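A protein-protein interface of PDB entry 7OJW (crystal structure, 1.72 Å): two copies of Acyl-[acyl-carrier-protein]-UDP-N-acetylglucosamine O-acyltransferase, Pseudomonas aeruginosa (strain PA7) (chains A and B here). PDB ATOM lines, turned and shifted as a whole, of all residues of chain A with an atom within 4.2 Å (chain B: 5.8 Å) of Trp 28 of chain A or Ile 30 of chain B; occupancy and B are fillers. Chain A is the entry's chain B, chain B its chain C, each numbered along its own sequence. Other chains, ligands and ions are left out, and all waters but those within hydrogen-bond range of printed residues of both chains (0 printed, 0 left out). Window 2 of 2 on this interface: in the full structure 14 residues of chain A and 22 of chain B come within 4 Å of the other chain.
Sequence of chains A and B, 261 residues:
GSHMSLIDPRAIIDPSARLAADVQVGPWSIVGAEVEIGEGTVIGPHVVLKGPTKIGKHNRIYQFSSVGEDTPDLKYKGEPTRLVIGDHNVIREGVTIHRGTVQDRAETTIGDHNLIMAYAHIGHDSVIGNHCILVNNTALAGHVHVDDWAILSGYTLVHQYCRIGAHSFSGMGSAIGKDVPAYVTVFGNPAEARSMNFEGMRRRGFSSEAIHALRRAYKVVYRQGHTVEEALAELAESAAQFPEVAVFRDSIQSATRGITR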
ATOM      1  N   ARG A  10      24.572   4.199  31.451  1.00  0.00           N
ATOM      2  CA  ARG A  10      23.712   5.399  31.323  1.00  0.00           C
ATOM      3  C   ARG A  10      22.745   5.591  32.504  1.00  0.00           C
ATOM      4  O   ARG A  10      22.055   6.607  32.584  1.00  0.00           O
ATOM      5  CB  ARG A  10      22.965   5.391  29.990  1.00  0.00           C
ATOM      6  CG  ARG A  10      23.906   5.544  28.799  1.00  0.00           C
ATOM      7  CD  ARG A  10      23.295   5.000  27.518  1.00  0.00           C
ATOM      8  NE  ARG A  10      23.098   3.547  27.590  1.00  0.00           N
ATOM      9  CZ  ARG A  10      22.898   2.764  26.539  1.00  0.00           C
ATOM     10  NH1 ARG A  10      22.844   3.283  25.319  1.00  0.00           N
ATOM     11  NH2 ARG A  10      22.729   1.456  26.699  1.00  0.00           N
ATOM     12  N   ALA A  11      22.716   4.636  33.425  1.00  0.00           N
ATOM     13  CA  ALA A  11      21.929   4.755  34.649  1.00  0.00           C
ATOM     14  C   ALA A  11      22.737   5.549  35.678  1.00  0.00           C
ATOM     15  O   ALA A  11      23.971   5.580  35.612  1.00  0.00           O
ATOM     16  CB  ALA A  11      21.605   3.377  35.208  1.00  0.00           C
ATOM     17  N   GLY A  26      18.498  -0.821  33.794  1.00  0.00           N
ATOM     18  CA  GLY A  26      18.477  -0.300  32.423  1.00  0.00           C
ATOM     19  C   GLY A  26      18.972   1.140  32.282  1.00  0.00           C
ATOM     20  O   GLY A  26      19.208   1.849  33.269  1.00  0.00           O
ATOM     21  N   PRO A  27      19.097   1.626  31.039  1.00  0.00           N
ATOM     22  CA  PRO A  27      19.652   2.976  30.830  1.00  0.00           C
ATOM     23  C   PRO A  27      18.710   4.070  31.328  1.00  0.00           C
ATOM     24  O   PRO A  27      17.497   3.929  31.295  1.00  0.00           O
ATOM     25  CB  PRO A  27      19.818   3.056  29.303  1.00  0.00           C
ATOM     26  CG  PRO A  27      18.761   2.068  28.766  1.00  0.00           C
ATOM     27  CD  PRO A  27      18.892   0.930  29.748  1.00  0.00           C
ATOM     28  N   TRP A  28      19.284   5.181  31.769  1.00  0.00           N
ATOM     29  CA  TRP A  28      18.538   6.355  32.210  1.00  0.00           C
ATOM     30  C   TRP A  28      17.622   6.095  33.417  1.00  0.00           C
ATOM     31  O   TRP A  28      16.610   6.792  33.597  1.00  0.00           O
ATOM     32  CB  TRP A  28      17.757   7.011  31.043  1.00  0.00           C
ATOM     33  CG  TRP A  28      18.486   6.993  29.743  1.00  0.00           C
ATOM     34  CD1 TRP A  28      19.676   7.597  29.449  1.00  0.00           C
ATOM     35  CD2 TRP A  28      18.108   6.257  28.578  1.00  0.00           C
ATOM     36  NE1 TRP A  28      20.046   7.304  28.155  1.00  0.00           N
ATOM     37  CE2 TRP A  28      19.088   6.497  27.593  1.00  0.00           C
ATOM     38  CE3 TRP A  28      17.032   5.405  28.273  1.00  0.00           C
ATOM     39  CZ2 TRP A  28      19.032   5.908  26.325  1.00  0.00           C
ATOM     40  CZ3 TRP A  28      16.934   4.895  26.989  1.00  0.00           C
ATOM     41  CH2 TRP A  28      17.931   5.133  26.043  1.00  0.00           C
ATOM     42  N   SER A  29      18.001   5.111  34.260  1.00  0.00           N
ATOM     43  CA  SER A  29      17.285   4.856  35.505  1.00  0.00           C
ATOM     44  C   SER A  29      18.093   5.499  36.597  1.00  0.00           C
ATOM     45  O   SER A  29      19.311   5.699  36.436  1.00  0.00           O
ATOM     46  CB  SER A  29      17.104   3.366  35.742  1.00  0.00           C
ATOM     47  OG  SER A  29      16.128   2.931  34.812  1.00  0.00           O
ATOM     48  N   PRO A  45      14.509   0.493  31.957  1.00  0.00           N
ATOM     49  CA  PRO A  45      15.027   1.850  31.703  1.00  0.00           C
ATOM     50  C   PRO A  45      14.066   2.910  32.219  1.00  0.00           C
ATOM     51  O   PRO A  45      12.896   2.598  32.408  1.00  0.00           O
ATOM     52  CB  PRO A  45      15.073   1.897  30.168  1.00  0.00           C
ATOM     53  CG  PRO A  45      13.855   1.058  29.751  1.00  0.00           C
ATOM     54  CD  PRO A  45      13.786  -0.057  30.782  1.00  0.00           C
ATOM     55  N   HIS A  46      14.512   4.182  32.396  1.00  0.00           N
ATOM     56  CA  HIS A  46      13.595   5.257  32.794  1.00  0.00           C
ATOM     57  C   HIS A  46      12.846   5.006  34.097  1.00  0.00           C
ATOM     58  O   HIS A  46      11.683   5.406  34.214  1.00  0.00           O
ATOM     59  CB  HIS A  46      12.594   5.537  31.666  1.00  0.00           C
ATOM     60  CG  HIS A  46      13.207   5.946  30.369  1.00  0.00           C
ATOM     61  ND1 HIS A  46      13.965   7.080  30.264  1.00  0.00           N
ATOM     62  CD2 HIS A  46      13.071   5.397  29.141  1.00  0.00           C
ATOM     63  CE1 HIS A  46      14.306   7.166  28.989  1.00  0.00           C
ATOM     64  NE2 HIS A  46      13.776   6.178  28.284  1.00  0.00           N
ATOM     65  N   ARG B  10      21.509   9.647  21.002  1.00  0.00           N
ATOM     66  CA  ARG B  10      21.195   9.185  22.353  1.00  0.00           C
ATOM     67  C   ARG B  10      20.054   8.145  22.348  1.00  0.00           C
ATOM     68  O   ARG B  10      19.652   7.692  23.410  1.00  0.00           O
ATOM     69  CB  ARG B  10      20.833  10.360  23.270  1.00  0.00           C
ATOM     70  CG  ARG B  10      22.031  11.262  23.570  1.00  0.00           C
ATOM     71  CD  ARG B  10      21.572  12.668  23.986  1.00  0.00           C
ATOM     72  NE  ARG B  10      20.916  13.360  22.871  1.00  0.00           N
ATOM     73  CZ  ARG B  10      20.780  14.678  22.766  1.00  0.00           C
ATOM     74  NH1 ARG B  10      21.237  15.479  23.722  1.00  0.00           N
ATOM     75  NH2 ARG B  10      20.163  15.206  21.716  1.00  0.00           N
ATOM     76  N   ALA B  11      19.525   7.798  21.168  1.00  0.00           N
ATOM     77  CA  ALA B  11      18.499   6.747  21.043  1.00  0.00           C
ATOM     78  C   ALA B  11      19.204   5.389  20.901  1.00  0.00           C
ATOM     79  O   ALA B  11      20.379   5.328  20.501  1.00  0.00           O
ATOM     80  CB  ALA B  11      17.626   6.993  19.821  1.00  0.00           C
ATOM     81  N   ILE B  12      18.462   4.301  21.170  1.00  0.00           N
ATOM     82  CA  ILE B  12      18.975   2.944  21.041  1.00  0.00           C
ATOM     83  C   ILE B  12      18.149   2.274  19.981  1.00  0.00           C
ATOM     84  O   ILE B  12      16.932   2.210  20.127  1.00  0.00           O
ATOM     85  CB  ILE B  12      18.912   2.166  22.385  1.00  0.00           C
ATOM     86  CG1 ILE B  12      19.756   2.869  23.456  1.00  0.00           C
ATOM     87  CG2 ILE B  12      19.325   0.671  22.175  1.00  0.00           C
ATOM     88  CD1 ILE B  12      19.671   2.217  24.854  1.00  0.00           C
ATOM     89  N   ILE B  13      18.799   1.862  18.869  1.00  0.00           N
ATOM     90  CA  ILE B  13      18.101   1.178  17.768  1.00  0.00           C
ATOM     91  C   ILE B  13      18.645  -0.234  17.735  1.00  0.00           C
ATOM     92  O   ILE B  13      19.834  -0.413  17.436  1.00  0.00           O
ATOM     93  CB  ILE B  13      18.337   1.874  16.395  1.00  0.00           C
ATOM     94  CG1 ILE B  13      18.110   3.437  16.441  1.00  0.00           C
ATOM     95  CG2 ILE B  13      17.478   1.185  15.295  1.00  0.00           C
ATOM     96  CD1 ILE B  13      16.732   3.904  16.871  1.00  0.00           C
ATOM     97  N   VAL B  25      13.887   9.562  15.223  1.00  0.00           N
ATOM     98  CA  VAL B  25      13.806   8.982  16.585  1.00  0.00           C
ATOM     99  C   VAL B  25      14.467   9.962  17.527  1.00  0.00           C
ATOM    100  O   VAL B  25      15.631  10.314  17.331  1.00  0.00           O
ATOM    101  CB  VAL B  25      14.420   7.575  16.690  1.00  0.00           C
ATOM    102  CG1 VAL B  25      14.332   7.055  18.139  1.00  0.00           C
ATOM    103  CG2 VAL B  25      13.733   6.597  15.726  1.00  0.00           C
ATOM    104  N   TRP B  28      16.951   9.309  23.917  1.00  0.00           N
ATOM    105  CA  TRP B  28      16.563   8.379  24.977  1.00  0.00           C
ATOM    106  C   TRP B  28      15.351   7.496  24.647  1.00  0.00           C
ATOM    107  O   TRP B  28      14.634   7.076  25.553  1.00  0.00           O
ATOM    108  CB  TRP B  28      16.359   9.124  26.305  1.00  0.00           C
ATOM    109  CG  TRP B  28      17.350  10.222  26.507  1.00  0.00           C
ATOM    110  CD1 TRP B  28      18.697  10.103  26.662  1.00  0.00           C
ATOM    111  CD2 TRP B  28      17.061  11.633  26.525  1.00  0.00           C
ATOM    112  NE1 TRP B  28      19.271  11.352  26.771  1.00  0.00           N
ATOM    113  CE2 TRP B  28      18.280  12.307  26.740  1.00  0.00           C
ATOM    114  CE3 TRP B  28      15.867  12.385  26.449  1.00  0.00           C
ATOM    115  CZ2 TRP B  28      18.362  13.712  26.785  1.00  0.00           C
ATOM    116  CZ3 TRP B  28      15.938  13.776  26.565  1.00  0.00           C
ATOM    117  CH2 TRP B  28      17.172  14.420  26.724  1.00  0.00           C
ATOM    118  N   SER B  29      15.131   7.225  23.355  1.00  0.00           N
ATOM    119  CA  SER B  29      14.072   6.321  22.915  1.00  0.00           C
ATOM    120  C   SER B  29      14.723   4.991  22.559  1.00  0.00           C
ATOM    121  O   SER B  29      15.895   4.967  22.177  1.00  0.00           O
ATOM    122  CB  SER B  29      13.314   6.894  21.730  1.00  0.00           C
ATOM    123  OG  SER B  29      12.494   7.948  22.218  1.00  0.00           O
ATOM    124  N   ILE B  30      13.973   3.895  22.705  1.00  0.00           N
ATOM    125  CA  ILE B  30      14.483   2.558  22.420  1.00  0.00           C
ATOM    126  C   ILE B  30      13.608   1.969  21.367  1.00  0.00           C
ATOM    127  O   ILE B  30      12.390   1.908  21.561  1.00  0.00           O
ATOM    128  CB  ILE B  30      14.422   1.703  23.705  1.00  0.00           C
ATOM    129  CG1 ILE B  30      15.363   2.256  24.751  1.00  0.00           C
ATOM    130  CG2 ILE B  30      14.670   0.180  23.418  1.00  0.00           C
ATOM    131  CD1 ILE B  30      15.126   1.611  26.152  1.00  0.00           C
ATOM    132  N   VAL B  31      14.216   1.614  20.224  1.00  0.00           N
ATOM    133  CA  VAL B  31      13.511   0.933  19.138  1.00  0.00           C
ATOM    134  C   VAL B  31      14.021  -0.510  19.298  1.00  0.00           C
ATOM    135  O   VAL B  31      15.162  -0.832  18.931  1.00  0.00           O
ATOM    136  CB  VAL B  31      13.800   1.534  17.757  1.00  0.00           C
ATOM    137  CG1 VAL B  31      13.185   0.668  16.652  1.00  0.00           C
ATOM    138  CG2 VAL B  31      13.306   2.978  17.675  1.00  0.00           C
ATOM    139  N   GLY B  32      13.188  -1.345  19.889  1.00  0.00           N
ATOM    140  CA  GLY B  32      13.546  -2.708  20.275  1.00  0.00           C
ATOM    141  C   GLY B  32      13.741  -3.674  19.134  1.00  0.00           C
ATOM    142  O   GLY B  32      13.547  -3.323  17.964  1.00  0.00           O
ATOM    143  N   VAL B  47      10.620   7.233  24.346  1.00  0.00           N
ATOM    144  CA  VAL B  47       9.617   6.260  23.900  1.00  0.00           C
ATOM    145  C   VAL B  47      10.213   4.855  23.981  1.00  0.00           C
ATOM    146  O   VAL B  47      11.375   4.669  23.621  1.00  0.00           O
ATOM    147  CB  VAL B  47       9.144   6.588  22.459  1.00  0.00           C
ATOM    148  CG1 VAL B  47       8.262   5.479  21.889  1.00  0.00           C
ATOM    149  CG2 VAL B  47       8.440   7.959  22.409  1.00  0.00           C
ATOM    150  N   VAL B  48       9.404   3.853  24.355  1.00  0.00           N
ATOM    151  CA  VAL B  48       9.877   2.459  24.366  1.00  0.00           C
ATOM    152  C   VAL B  48       9.046   1.709  23.360  1.00  0.00           C
ATOM    153  O   VAL B  48       7.820   1.622  23.516  1.00  0.00           O
ATOM    154  CB  VAL B  48       9.818   1.796  25.769  1.00  0.00           C
ATOM    155  CG1 VAL B  48      10.180   0.292  25.696  1.00  0.00           C
ATOM    156  CG2 VAL B  48      10.715   2.536  26.755  1.00  0.00           C
ATOM    157  N   LEU B  49       9.707   1.160  22.337  1.00  0.00           N
ATOM    158  CA  LEU B  49       9.047   0.341  21.327  1.00  0.00           C
ATOM    159  C   LEU B  49       9.582  -1.069  21.473  1.00  0.00           C
ATOM    160  O   LEU B  49      10.810  -1.268  21.468  1.00  0.00           O
ATOM    161  CB  LEU B  49       9.328   0.824  19.892  1.00  0.00           C
ATOM    162  CG  LEU B  49       9.007   2.269  19.536  1.00  0.00           C
ATOM    163  CD1 LEU B  49       9.269   2.499  18.003  1.00  0.00           C
ATOM    164  CD2 LEU B  49       7.541   2.605  19.855  1.00  0.00           C
ATOM    165  N   LYS B  50       8.683  -2.049  21.558  1.00  0.00           N
ATOM    166  CA  LYS B  50       9.091  -3.447  21.697  1.00  0.00           C
ATOM    167  C   LYS B  50       8.403  -4.227  20.584  1.00  0.00           C
ATOM    168  O   LYS B  50       7.367  -3.779  20.057  1.00  0.00           O
ATOM    169  CB  LYS B  50       8.697  -3.934  23.119  1.00  0.00           C
ATOM    170  CG  LYS B  50       9.213  -5.327  23.458  1.00  0.00           C
ATOM    171  CD  LYS B  50       8.909  -5.712  24.912  1.00  0.00           C
ATOM    172  CE  LYS B  50       9.473  -7.075  25.256  1.00  0.00           C
ATOM    173  NZ  LYS B  50       9.163  -7.444  26.659  1.00  0.00           N
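Trp 28 of chain A touches Arg 10 of chain B, but with the chains exchanged Arg 10 of chain A does not touch Trp 28 of chain B (6.9 Å). Trp 28 of chain A touches its own counterpart, Trp 28 of chain B. Positions printed for both chains: 10, 11, 28 and 29. Of the 7 pairs that touch across the chains among the printed residues, 1 has its exchanged pair printed and touching as well.
NE2 of His 46 of chain A sits at hydrogen-bond distance from O of Trp 28 of chain B (3.0 Å).
NH1 of Arg 10 of chain A touches CD1 of Ile 12 of chain B, at 3.4 Å. Trp 28 of chain A touches Arg 10 of chain B. CD1 of Ile 12 of chain B touches CH2 of Trp 28 of chain A, at 3.6 Å. Trp 28 of chain A touches Trp 28 of chain B (NE1 to CD1, 3.4 Å). CZ3 of Trp 28 of chain A touches CG1 of Ile 30 of chain B, at 3.8 Å. CD1 of Ile 30 of chain B touches CG of Pro 45 of chain A, at 3.9 Å.
The backbone NH (N) of His 46 of chain A lies within hydrogen-bond range of the side-chain hydroxyl (OG) of Ser 29 of chain A, at 3.2 Å. N of Trp 28 of chain B sits at hydrogen-bond distance from O of Arg 10 of chain B, at 3.2 Å. N of Ile 12 of chain B is in hydrogen-bond range of O of Ser 29 of chain B (2.8 Å). O of Ile 12 of chain B sits at hydrogen-bond distance from N of Val 31 of chain B (2.8 Å). N of Ile 30 of chain B sits at hydrogen-bond distance from O of Val 47 of chain B, 2.9 Å away. The backbone carbonyl oxygen of Ile 30 of chain B is in hydrogen-bond range of the backbone NH of Leu 49 of chain B (2.9 Å).
Of the printed residues of chain B, Arg 10 of chain A touches Ile 12. Of chain B, only Arg 10, Ile 12, Trp 28 and Ile 30 come within 4 Å of Trp 28 of chain A. Printed residues of chain B within 4 Å of Pro 45 of chain A: Ile 30 (3.9 Å). Of the printed residues of chain B, His 46 of chain A touches Trp 28. Printed residues of chain A within 4 Å of Trp 28 of chain B: Trp 28 and His 46. Ile 30 of chain B touches just these residues of chain A: Trp 28 and Pro 45. Val 31 of chain B touches none of the printed residues of chain A. The nearest printed residue of chain A that does not touch Ile 30 of chain B is Pro 27 of chain A (4.5 Å).
Hydrophobic or aromatic side chains of chain B that line the printed part of chain A: Ile 12, Trp 28 and Ile 30. Along chain B the printed residues that touch a printed residue of chain A span positions 10 to 30. Among the printed residues, 7 pairs touch across the chains. Among the printed residues, no Asp or Glu carboxylate lies within 4 Å of a Lys or Arg side-chain nitrogen of the other chain.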
